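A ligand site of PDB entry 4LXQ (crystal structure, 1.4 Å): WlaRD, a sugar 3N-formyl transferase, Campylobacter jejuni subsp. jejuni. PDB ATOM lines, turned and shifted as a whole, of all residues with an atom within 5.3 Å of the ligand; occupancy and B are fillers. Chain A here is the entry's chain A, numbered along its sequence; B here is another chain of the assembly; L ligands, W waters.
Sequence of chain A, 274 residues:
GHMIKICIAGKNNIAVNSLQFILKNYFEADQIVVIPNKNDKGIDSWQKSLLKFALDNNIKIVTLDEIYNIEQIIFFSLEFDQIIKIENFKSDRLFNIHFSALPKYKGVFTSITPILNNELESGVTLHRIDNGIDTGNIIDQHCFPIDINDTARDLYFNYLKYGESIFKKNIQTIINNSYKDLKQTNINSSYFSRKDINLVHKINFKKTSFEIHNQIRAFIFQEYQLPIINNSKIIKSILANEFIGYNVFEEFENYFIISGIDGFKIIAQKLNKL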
ATOM      1  N   SER A  77      14.281  12.742 -20.224  1.00  0.00           N
ATOM      2  CA  SER A  77      13.841  13.393 -21.461  1.00  0.00           C
ATOM      3  C   SER A  77      13.314  12.340 -22.442  1.00  0.00           C
ATOM      4  O   SER A  77      13.992  11.345 -22.768  1.00  0.00           O
ATOM      5  CB  SER A  77      15.037  14.104 -22.073  1.00  0.00           C
ATOM      6  OG  SER A  77      14.808  14.356 -23.462  1.00  0.00           O
ATOM      7  N   PHE A  80      12.056  15.627 -25.366  1.00  0.00           N
ATOM      8  CA  PHE A  80      12.142  16.997 -24.845  1.00  0.00           C
ATOM      9  C   PHE A  80      12.904  17.944 -25.775  1.00  0.00           C
ATOM     10  O   PHE A  80      13.823  17.525 -26.504  1.00  0.00           O
ATOM     11  CB  PHE A  80      12.880  16.949 -23.481  1.00  0.00           C
ATOM     12  CG  PHE A  80      12.806  18.192 -22.644  1.00  0.00           C
ATOM     13  CD1 PHE A  80      13.958  18.593 -21.982  1.00  0.00           C
ATOM     14  CD2 PHE A  80      11.652  18.951 -22.478  1.00  0.00           C
ATOM     15  CE1 PHE A  80      13.966  19.708 -21.112  1.00  0.00           C
ATOM     16  CE2 PHE A  80      11.657  20.112 -21.639  1.00  0.00           C
ATOM     17  CZ  PHE A  80      12.811  20.470 -20.971  1.00  0.00           C
ATOM     18  N   ASP A  81      12.483  19.202 -25.745  1.00  0.00           N
ATOM     19  CA  ASP A  81      12.940  20.178 -26.730  1.00  0.00           C
ATOM     20  C   ASP A  81      13.989  21.117 -26.222  1.00  0.00           C
ATOM     21  O   ASP A  81      14.393  21.961 -27.007  1.00  0.00           O
ATOM     22  CB  ASP A  81      11.750  20.925 -27.346  1.00  0.00           C
ATOM     23  CG  ASP A  81      10.926  21.668 -26.322  1.00  0.00           C
ATOM     24  OD1 ASP A  81       9.923  22.343 -26.704  1.00  0.00           O
ATOM     25  OD2 ASP A  81      11.198  21.680 -25.099  1.00  0.00           O
ATOM     26  N   GLN A  82      14.445  21.026 -24.971  1.00  0.00           N
ATOM     27  CA  GLN A  82      15.475  21.969 -24.478  1.00  0.00           C
ATOM     28  C   GLN A  82      16.778  21.264 -24.154  1.00  0.00           C
ATOM     29  O   GLN A  82      16.744  20.243 -23.474  1.00  0.00           O
ATOM     30  CB  GLN A  82      14.999  22.649 -23.197  1.00  0.00           C
ATOM     31  CG  GLN A  82      13.668  23.430 -23.329  1.00  0.00           C
ATOM     32  CD  GLN A  82      13.383  24.181 -22.061  1.00  0.00           C
ATOM     33  OE1 GLN A  82      14.221  25.007 -21.678  1.00  0.00           O
ATOM     34  NE2 GLN A  82      12.275  23.906 -21.382  1.00  0.00           N
ATOM     35  N   ILE A  83      17.918  21.770 -24.626  1.00  0.00           N
ATOM     36  CA  ILE A  83      19.223  21.254 -24.228  1.00  0.00           C
ATOM     37  C   ILE A  83      19.489  21.656 -22.771  1.00  0.00           C
ATOM     38  O   ILE A  83      19.306  22.809 -22.390  1.00  0.00           O
ATOM     39  CB  ILE A  83      20.322  21.810 -25.146  1.00  0.00           C
ATOM     40  CG1 ILE A  83      20.118  21.313 -26.589  1.00  0.00           C
ATOM     41  CG2 ILE A  83      21.736  21.448 -24.604  1.00  0.00           C
ATOM     42  CD1 ILE A  83      20.615  19.878 -26.739  1.00  0.00           C
ATOM     43  N   ILE A  84      19.855  20.678 -21.955  1.00  0.00           N
ATOM     44  CA  ILE A  84      20.213  20.966 -20.573  1.00  0.00           C
ATOM     45  C   ILE A  84      21.718  21.059 -20.429  1.00  0.00           C
ATOM     46  O   ILE A  84      22.499  20.531 -21.234  1.00  0.00           O
ATOM     47  CB  ILE A  84      19.586  19.980 -19.605  1.00  0.00           C
ATOM     48  CG1 ILE A  84      20.178  18.568 -19.772  1.00  0.00           C
ATOM     49  CG2 ILE A  84      18.048  19.961 -19.669  1.00  0.00           C
ATOM     50  CD1 ILE A  84      19.904  17.627 -18.543  1.00  0.00           C
ATOM     51  N   LYS A  85      22.132  21.727 -19.361  1.00  0.00           N
ATOM     52  CA  LYS A  85      23.538  21.795 -18.961  1.00  0.00           C
ATOM     53  C   LYS A  85      23.645  21.032 -17.656  1.00  0.00           C
ATOM     54  O   LYS A  85      22.952  21.355 -16.662  1.00  0.00           O
ATOM     55  CB  LYS A  85      23.941  23.260 -18.781  1.00  0.00           C
ATOM     56  CG  LYS A  85      23.825  24.062 -20.062  1.00  0.00           C
ATOM     57  CD  LYS A  85      24.001  25.550 -19.799  1.00  0.00           C
ATOM     58  CE  LYS A  85      23.786  26.387 -21.055  1.00  0.00           C
ATOM     59  NZ  LYS A  85      23.261  27.700 -20.597  1.00  0.00           N
ATOM     60  N   ASN A  96      18.043  10.208 -21.438  1.00  0.00           N
ATOM     61  CA  ASN A  96      17.283  10.519 -22.652  1.00  0.00           C
ATOM     62  C   ASN A  96      17.110   9.226 -23.416  1.00  0.00           C
ATOM     63  O   ASN A  96      17.950   8.323 -23.438  1.00  0.00           O
ATOM     64  CB  ASN A  96      18.094  11.530 -23.498  1.00  0.00           C
ATOM     65  CG  ASN A  96      17.417  11.874 -24.813  1.00  0.00           C
ATOM     66  OD1 ASN A  96      17.954  11.627 -25.929  1.00  0.00           O
ATOM     67  ND2 ASN A  96      16.272  12.425 -24.701  1.00  0.00           N
ATOM     68  N   HIS A  98      16.896   8.547 -27.326  1.00  0.00           N
ATOM     69  CA  HIS A  98      17.098   9.211 -28.624  1.00  0.00           C
ATOM     70  C   HIS A  98      16.612   8.292 -29.724  1.00  0.00           C
ATOM     71  O   HIS A  98      16.853   7.090 -29.711  1.00  0.00           O
ATOM     72  CB  HIS A  98      18.584   9.539 -28.836  1.00  0.00           C
ATOM     73  CG  HIS A  98      18.852  10.181 -30.160  1.00  0.00           C
ATOM     74  ND1 HIS A  98      18.425  11.458 -30.449  1.00  0.00           N
ATOM     75  CD2 HIS A  98      19.474   9.698 -31.252  1.00  0.00           C
ATOM     76  CE1 HIS A  98      18.791  11.750 -31.697  1.00  0.00           C
ATOM     77  NE2 HIS A  98      19.444  10.709 -32.189  1.00  0.00           N
ATOM     78  N   GLY A 107      21.349  14.498 -33.339  1.00  0.00           N
ATOM     79  CA  GLY A 107      20.719  15.742 -33.804  1.00  0.00           C
ATOM     80  C   GLY A 107      19.232  15.520 -34.051  1.00  0.00           C
ATOM     81  O   GLY A 107      18.561  14.815 -33.261  1.00  0.00           O
ATOM     82  N   VAL A 108      18.721  16.133 -35.127  1.00  0.00           N
ATOM     83  CA  VAL A 108      17.279  16.267 -35.254  1.00  0.00           C
ATOM     84  C   VAL A 108      16.742  15.587 -36.521  1.00  0.00           C
ATOM     85  O   VAL A 108      17.500  15.029 -37.324  1.00  0.00           O
ATOM     86  CB  VAL A 108      16.892  17.773 -35.300  1.00  0.00           C
ATOM     87  CG1 VAL A 108      17.299  18.429 -33.956  1.00  0.00           C
ATOM     88  CG2 VAL A 108      17.561  18.492 -36.444  1.00  0.00           C
ATOM     89  N   HIS A 127      20.314   6.649 -23.226  1.00  0.00           N
ATOM     90  CA  HIS A 127      21.657   7.064 -22.879  1.00  0.00           C
ATOM     91  C   HIS A 127      21.632   8.080 -21.736  1.00  0.00           C
ATOM     92  O   HIS A 127      20.599   8.701 -21.468  1.00  0.00           O
ATOM     93  CB  HIS A 127      22.380   7.612 -24.141  1.00  0.00           C
ATOM     94  CG  HIS A 127      21.744   8.856 -24.700  1.00  0.00           C
ATOM     95  ND1 HIS A 127      22.173  10.105 -24.336  1.00  0.00           N
ATOM     96  CD2 HIS A 127      20.765   9.042 -25.622  1.00  0.00           C
ATOM     97  CE1 HIS A 127      21.438  11.024 -24.950  1.00  0.00           C
ATOM     98  NE2 HIS A 127      20.611  10.400 -25.775  1.00  0.00           N
ATOM     99  N   ILE A 129      22.391  11.696 -20.291  1.00  0.00           N
ATOM    100  CA  ILE A 129      22.558  13.015 -20.873  1.00  0.00           C
ATOM    101  C   ILE A 129      23.899  13.586 -20.437  1.00  0.00           C
ATOM    102  O   ILE A 129      24.190  13.633 -19.222  1.00  0.00           O
ATOM    103  CB  ILE A 129      21.447  13.985 -20.439  1.00  0.00           C
ATOM    104  CG1 ILE A 129      20.110  13.491 -20.997  1.00  0.00           C
ATOM    105  CG2 ILE A 129      21.744  15.437 -20.879  1.00  0.00           C
ATOM    106  CD1 ILE A 129      18.938  14.308 -20.560  1.00  0.00           C
ATOM    107  N   ASP A 130      24.742  13.992 -21.373  1.00  0.00           N
ATOM    108  CA  ASP A 130      25.902  14.831 -21.051  1.00  0.00           C
ATOM    109  C   ASP A 130      25.730  16.170 -21.748  1.00  0.00           C
ATOM    110  O   ASP A 130      24.626  16.471 -22.266  1.00  0.00           O
ATOM    111  CB  ASP A 130      27.229  14.136 -21.382  1.00  0.00           C
ATOM    112  CG  ASP A 130      27.446  13.874 -22.864  1.00  0.00           C
ATOM    113  OD1 ASP A 130      28.352  13.046 -23.141  1.00  0.00           O
ATOM    114  OD2 ASP A 130      26.752  14.488 -23.672  1.00  0.00           O
ATOM    115  N   ASN A 131      26.709  17.077 -21.754  1.00  0.00           N
ATOM    116  CA  ASN A 131      26.478  18.410 -22.269  1.00  0.00           C
ATOM    117  C   ASN A 131      26.357  18.514 -23.785  1.00  0.00           C
ATOM    118  O   ASN A 131      25.900  19.543 -24.254  1.00  0.00           O
ATOM    119  CB  ASN A 131      27.550  19.366 -21.744  1.00  0.00           C
ATOM    120  CG  ASN A 131      27.254  19.791 -20.351  1.00  0.00           C
ATOM    121  OD1 ASN A 131      26.111  19.837 -19.918  1.00  0.00           O
ATOM    122  ND2 ASN A 131      28.303  20.100 -19.600  1.00  0.00           N
ATOM    123  N   GLY A 132      26.745  17.458 -24.503  1.00  0.00           N
ATOM    124  CA  GLY A 132      26.610  17.465 -25.995  1.00  0.00           C
ATOM    125  C   GLY A 132      25.273  16.929 -26.447  1.00  0.00           C
ATOM    126  O   GLY A 132      24.465  16.447 -25.649  1.00  0.00           O
ATOM    127  N   ILE A 133      25.054  17.020 -27.766  1.00  0.00           N
ATOM    128  CA  ILE A 133      23.786  16.616 -28.370  1.00  0.00           C
ATOM    129  C   ILE A 133      23.801  15.122 -28.682  1.00  0.00           C
ATOM    130  O   ILE A 133      24.492  14.658 -29.611  1.00  0.00           O
ATOM    131  CB  ILE A 133      23.505  17.450 -29.621  1.00  0.00           C
ATOM    132  CG1 ILE A 133      23.436  18.922 -29.241  1.00  0.00           C
ATOM    133  CG2 ILE A 133      22.202  16.933 -30.301  1.00  0.00           C
ATOM    134  CD1 ILE A 133      23.178  19.862 -30.416  1.00  0.00           C
ATOM    135  N   ASP A 134      23.088  14.352 -27.882  1.00  0.00           N
ATOM    136  CA  ASP A 134      22.987  12.914 -28.014  1.00  0.00           C
ATOM    137  C   ASP A 134      24.303  12.159 -27.952  1.00  0.00           C
ATOM    138  O   ASP A 134      24.472  11.071 -28.525  1.00  0.00           O
ATOM    139  CB  ASP A 134      22.262  12.527 -29.329  1.00  0.00           C
ATOM    140  CG  ASP A 134      20.971  13.273 -29.511  1.00  0.00           C
ATOM    141  OD1 ASP A 134      20.204  13.424 -28.554  1.00  0.00           O
ATOM    142  OD2 ASP A 134      20.776  13.816 -30.631  1.00  0.00           O
ATOM    143  N   THR A 135      25.220  12.694 -27.123  1.00  0.00           N
ATOM    144  CA  THR A 135      26.617  12.229 -27.055  1.00  0.00           C
ATOM    145  C   THR A 135      26.885  11.338 -25.845  1.00  0.00           C
ATOM    146  O   THR A 135      27.937  10.703 -25.810  1.00  0.00           O
ATOM    147  CB  THR A 135      27.569  13.438 -27.087  1.00  0.00           C
ATOM    148  OG1 THR A 135      27.036  14.467 -26.258  1.00  0.00           O
ATOM    149  CG2 THR A 135      27.696  14.002 -28.514  1.00  0.00           C
ATOM    150  N   TYR A 191      25.741  13.340 -37.425  1.00  0.00           N
ATOM    151  CA  TYR A 191      24.956  14.415 -36.805  1.00  0.00           C
ATOM    152  C   TYR A 191      24.329  15.271 -37.897  1.00  0.00           C
ATOM    153  O   TYR A 191      24.983  15.619 -38.881  1.00  0.00           O
ATOM    154  CB  TYR A 191      25.838  15.274 -35.895  1.00  0.00           C
ATOM    155  CG  TYR A 191      25.196  16.560 -35.441  1.00  0.00           C
ATOM    156  CD1 TYR A 191      24.373  16.572 -34.330  1.00  0.00           C
ATOM    157  CD2 TYR A 191      25.376  17.770 -36.095  1.00  0.00           C
ATOM    158  CE1 TYR A 191      23.780  17.731 -33.883  1.00  0.00           C
ATOM    159  CE2 TYR A 191      24.821  18.949 -35.664  1.00  0.00           C
ATOM    160  CZ  TYR A 191      24.010  18.915 -34.528  1.00  0.00           C
ATOM    161  OH  TYR A 191      23.459  20.115 -34.111  1.00  0.00           O
ATOM    162  N   PHE A 192      23.058  15.598 -37.709  1.00  0.00           N
ATOM    163  CA  PHE A 192      22.361  16.556 -38.564  1.00  0.00           C
ATOM    164  C   PHE A 192      21.631  17.575 -37.738  1.00  0.00           C
ATOM    165  O   PHE A 192      20.917  17.256 -36.782  1.00  0.00           O
ATOM    166  CB  PHE A 192      21.380  15.836 -39.516  1.00  0.00           C
ATOM    167  CG  PHE A 192      22.072  14.876 -40.414  1.00  0.00           C
ATOM    168  CD1 PHE A 192      22.478  15.303 -41.681  1.00  0.00           C
ATOM    169  CD2 PHE A 192      22.388  13.598 -39.996  1.00  0.00           C
ATOM    170  CE1 PHE A 192      23.225  14.451 -42.487  1.00  0.00           C
ATOM    171  CE2 PHE A 192      23.164  12.739 -40.809  1.00  0.00           C
ATOM    172  CZ  PHE A 192      23.528  13.179 -42.072  1.00  0.00           C
ATOM    173  N   SER A 193      21.808  18.835 -38.136  1.00  0.00           N
ATOM    174  CA  SER A 193      21.083  19.946 -37.532  1.00  0.00           C
ATOM    175  C   SER A 193      19.914  20.409 -38.400  1.00  0.00           C
ATOM    176  O   SER A 193      19.795  19.978 -39.550  1.00  0.00           O
ATOM    177  CB  SER A 193      22.022  21.128 -37.297  1.00  0.00           C
ATOM    178  OG  SER A 193      22.336  21.670 -38.573  1.00  0.00           O
ATOM    179  N   ARG A 194      19.066  21.269 -37.858  1.00  0.00           N
ATOM    180  CA  ARG A 194      17.928  21.747 -38.632  1.00  0.00           C
ATOM    181  C   ARG A 194      18.352  22.445 -39.905  1.00  0.00           C
ATOM    182  O   ARG A 194      17.705  22.252 -40.927  1.00  0.00           O
ATOM    183  CB  ARG A 194      17.022  22.662 -37.787  1.00  0.00           C
ATOM    184  CG  ARG A 194      16.218  21.857 -36.798  1.00  0.00           C
ATOM    185  CD  ARG A 194      15.104  22.588 -36.027  1.00  0.00           C
ATOM    186  NE  ARG A 194      14.770  21.742 -34.870  1.00  0.00           N
ATOM    187  CZ  ARG A 194      15.257  21.914 -33.640  1.00  0.00           C
ATOM    188  NH1 ARG A 194      16.066  22.932 -33.362  1.00  0.00           N
ATOM    189  NH2 ARG A 194      14.913  21.063 -32.666  1.00  0.00           N
ATOM    190  N   LYS A 195      19.447  23.187 -39.899  1.00  0.00           N
ATOM    191  CA  LYS A 195      19.977  23.850 -41.103  1.00  0.00           C
ATOM    192  C   LYS A 195      20.409  22.868 -42.177  1.00  0.00           C
ATOM    193  O   LYS A 195      20.436  23.226 -43.359  1.00  0.00           O
ATOM    194  CB  LYS A 195      21.193  24.732 -40.745  1.00  0.00           C
ATOM    195  CG  LYS A 195      20.974  26.253 -40.840  1.00  0.00           C
ATOM    196  CD  LYS A 195      19.656  26.719 -40.213  1.00  0.00           C
ATOM    197  CE  LYS A 195      19.287  28.132 -40.672  1.00  0.00           C
ATOM    198  NZ  LYS A 195      19.322  28.333 -42.161  1.00  0.00           N
ATOM    199  N   LYS B 206      29.870  21.960 -38.051  1.00  0.00           N
ATOM    200  CA  LYS B 206      28.774  21.568 -37.138  1.00  0.00           C
ATOM    201  C   LYS B 206      28.355  20.132 -37.411  1.00  0.00           C
ATOM    202  O   LYS B 206      27.245  19.802 -37.837  1.00  0.00           O
ATOM    203  CB  LYS B 206      27.607  22.551 -37.256  1.00  0.00           C
ATOM    204  CG  LYS B 206      28.068  23.958 -36.846  1.00  0.00           C
ATOM    205  CD  LYS B 206      26.921  24.853 -36.370  1.00  0.00           C
ATOM    206  CE  LYS B 206      27.429  26.086 -35.638  1.00  0.00           C
ATOM    207  NZ  LYS B 206      27.995  27.012 -36.651  1.00  0.00           N
HETATM  208  N1  LIG L   1      20.324  18.050 -23.313  1.00  0.00           N
HETATM  209  C1  LIG L   1      21.567  17.676 -23.568  1.00  0.00           C
HETATM  210  N2  LIG L   1      22.584  18.325 -22.977  1.00  0.00           N
HETATM  211  N3  LIG L   1      21.916  16.645 -24.357  1.00  0.00           N
HETATM  212  C2  LIG L   1      20.926  15.954 -24.998  1.00  0.00           C
HETATM  213  O1  LIG L   1      21.395  14.891 -25.694  1.00  0.00           O
HETATM  214  C3  LIG L   1      19.592  16.276 -24.781  1.00  0.00           C
HETATM  215  N4  LIG L   1      18.473  15.801 -25.523  1.00  0.00           N
HETATM  216  C4  LIG L   1      17.242  16.620 -25.521  1.00  0.00           C
HETATM  217  C5  LIG L   1      16.945  16.953 -24.063  1.00  0.00           C
HETATM  218  N5  LIG L   1      18.106  17.735 -23.592  1.00  0.00           N
HETATM  219  C6  LIG L   1      19.350  17.336 -23.925  1.00  0.00           C
HETATM  220  C7  LIG L   1      17.236  17.901 -26.368  1.00  0.00           C
HETATM  221  N6  LIG L   1      17.689  17.687 -27.738  1.00  0.00           N
HETATM  222  C8  LIG L   1      18.357  20.856 -30.326  1.00  0.00           C
HETATM  223  C9  LIG L   1      17.689  21.067 -29.115  1.00  0.00           C
HETATM  224  C10 LIG L   1      17.425  20.005 -28.249  1.00  0.00           C
HETATM  225  C11 LIG L   1      17.915  18.741 -28.547  1.00  0.00           C
HETATM  226  C12 LIG L   1      18.559  18.514 -29.759  1.00  0.00           C
HETATM  227  C13 LIG L   1      18.815  19.575 -30.637  1.00  0.00           C
HETATM  228  C14 LIG L   1      18.641  22.029 -31.222  1.00  0.00           C
HETATM  229  O2  LIG L   1      18.199  23.128 -30.891  1.00  0.00           O
HETATM  230  N7  LIG L   1      19.440  21.859 -32.284  1.00  0.00           N
HETATM  231  C15 LIG L   1      19.792  23.005 -33.140  1.00  0.00           C
HETATM  232  C16 LIG L   1      21.309  23.173 -33.081  1.00  0.00           C
HETATM  233  C17 LIG L   1      21.757  23.648 -31.714  1.00  0.00           C
HETATM  234  C18 LIG L   1      23.237  23.951 -31.648  1.00  0.00           C
HETATM  235  O3  LIG L   1      23.992  23.859 -32.649  1.00  0.00           O
HETATM  236  O4  LIG L   1      23.681  24.271 -30.524  1.00  0.00           O
HETATM  237  C19 LIG L   1      19.474  22.787 -34.598  1.00  0.00           C
HETATM  238  O5  LIG L   1      19.420  21.636 -34.993  1.00  0.00           O
HETATM  239  O6  LIG L   1      19.344  23.751 -35.381  1.00  0.00           O
HETATM  240  C20 LIG L   1      18.556  14.856 -26.382  1.00  0.00           C
HETATM  241  O7  LIG L   1      17.592  14.623 -27.129  1.00  0.00           O
HETATM  242  O   HOH W   1      22.078  24.556 -28.345  1.00  0.00           O
HETATM  243  O   HOH W   2      16.808  25.239 -34.473  1.00  0.00           O
HETATM  244  O   HOH W   3      18.444  14.984 -30.384  1.00  0.00           O
HETATM  245  O   HOH W   4      24.008  13.760 -24.333  1.00  0.00           O
HETATM  246  O   HOH W   5      16.970  12.573 -28.507  1.00  0.00           O
HETATM  247  O   HOH W   6      20.801  19.554 -33.502  1.00  0.00           O
HETATM  248  O   HOH W   7      24.452  22.417 -34.977  1.00  0.00           O
HETATM  249  O   HOH W   8      16.136  15.990 -29.879  1.00  0.00           O
HETATM  250  O   HOH W   9      14.358  15.190 -27.988  1.00  0.00           O
HETATM  251  O   HOH W  10      20.626  24.400 -37.475  1.00  0.00           O
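The backbone carbonyl oxygen (O) of Gly 132 lies close to the side-chain hydroxyl (OG1) of Thr 135 (3.3 Å).
The backbone NH of Val 108 lies within hydrogen-bond range of the backbone carbonyl oxygen of Phe 192, 3.0 Å away.
OD1 of Asp 134 is in hydrogen-bond range of ND1 of His 98.
N of Gly 132 sits at hydrogen-bond distance from OD2 of Asp 130, 3.1 Å away.
ND2 of Asn 96 lies within hydrogen-bond range of OG of Ser 77.
The side-chain hydroxyl (OG1) of Thr 135 lies within hydrogen-bond range of the side-chain carboxylate (OD2) of Asp 130 (2.6 Å).
The side-chain carboxylate (OD2) of Asp 134 sits at hydrogen-bond distance from the backbone NH (N) of Gly 107 (2.9 Å).
The backbone NH (N) of His 127 sits at hydrogen-bond distance from the backbone carbonyl oxygen (O) of Asn 96.
Water W10 lies within hydrogen-bond range of an oxygen (O6) of the ligand, the backbone NH of Lys 195 and the side-chain hydroxyl of Ser 193.
Water W7 lies within hydrogen-bond range of the side-chain hydroxyl (OH) of Tyr 191 (2.7 Å) and an oxygen (O3) of the ligand (2.8 Å).
Water W6 bridges the side-chain hydroxyl of Tyr 191 (2.8 Å) and an oxygen (O5) of the ligand (2.9 Å).
Water W2 lies within hydrogen-bond range of NH1 of Arg 194 and O6 of the ligand.
Water W9 bridges O of Phe 80 (2.8 Å) and O7 of the ligand (3.4 Å).
O of Gln 82 is in hydrogen-bond range of N5 of the ligand.
An oxygen (O6) of the ligand is in salt-bridge range of the guanidinium group of Arg 194 (3.9 Å).
The backbone NH (N) of Ile 84 lies within hydrogen-bond range of a nitrogen (N1) of the ligand, 3.0 Å away.
An oxygen (O5) of the ligand lies within hydrogen-bond range of the backbone NH (N) of Arg 194, at 2.9 Å.
N2 of the ligand lies within hydrogen-bond range of O of Asp 130, at 2.8 Å.
The side-chain amide oxygen of Asn 96 lies close to an oxygen (O7) of the ligand (3.2 Å).
A nitrogen (N3) of the ligand sits close to the backbone carbonyl oxygen of Gly 132 (2.9 Å).
An oxygen (O1) of the ligand lies within hydrogen-bond range of the backbone NH (N) of Asp 134 (2.8 Å).
O of Ile 84 lies within hydrogen-bond range of N2 of the ligand (2.8 Å).
Merely in contact with the ligand: Ser 77 (3.4 Å), Phe 80 (3.4 Å), Asp 81 (3.8 Å), Ile 83 (3.4 Å), Val 108 (3.8 Å), His 127 (3.9 Å), Ile 129 (3.5 Å), Asn 131 (3.8 Å), Ile 133 (3.8 Å), Tyr 191 (3.9 Å) and Ser 193 (3.5 Å).
Hydrophobic or aromatic side chains that line the ligand: Phe 80, Ile 83, Ile 84, Val 108, His 127 and Ile 129.
Along chain A the residues within 4 Å of the ligand span positions 77 to 194.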
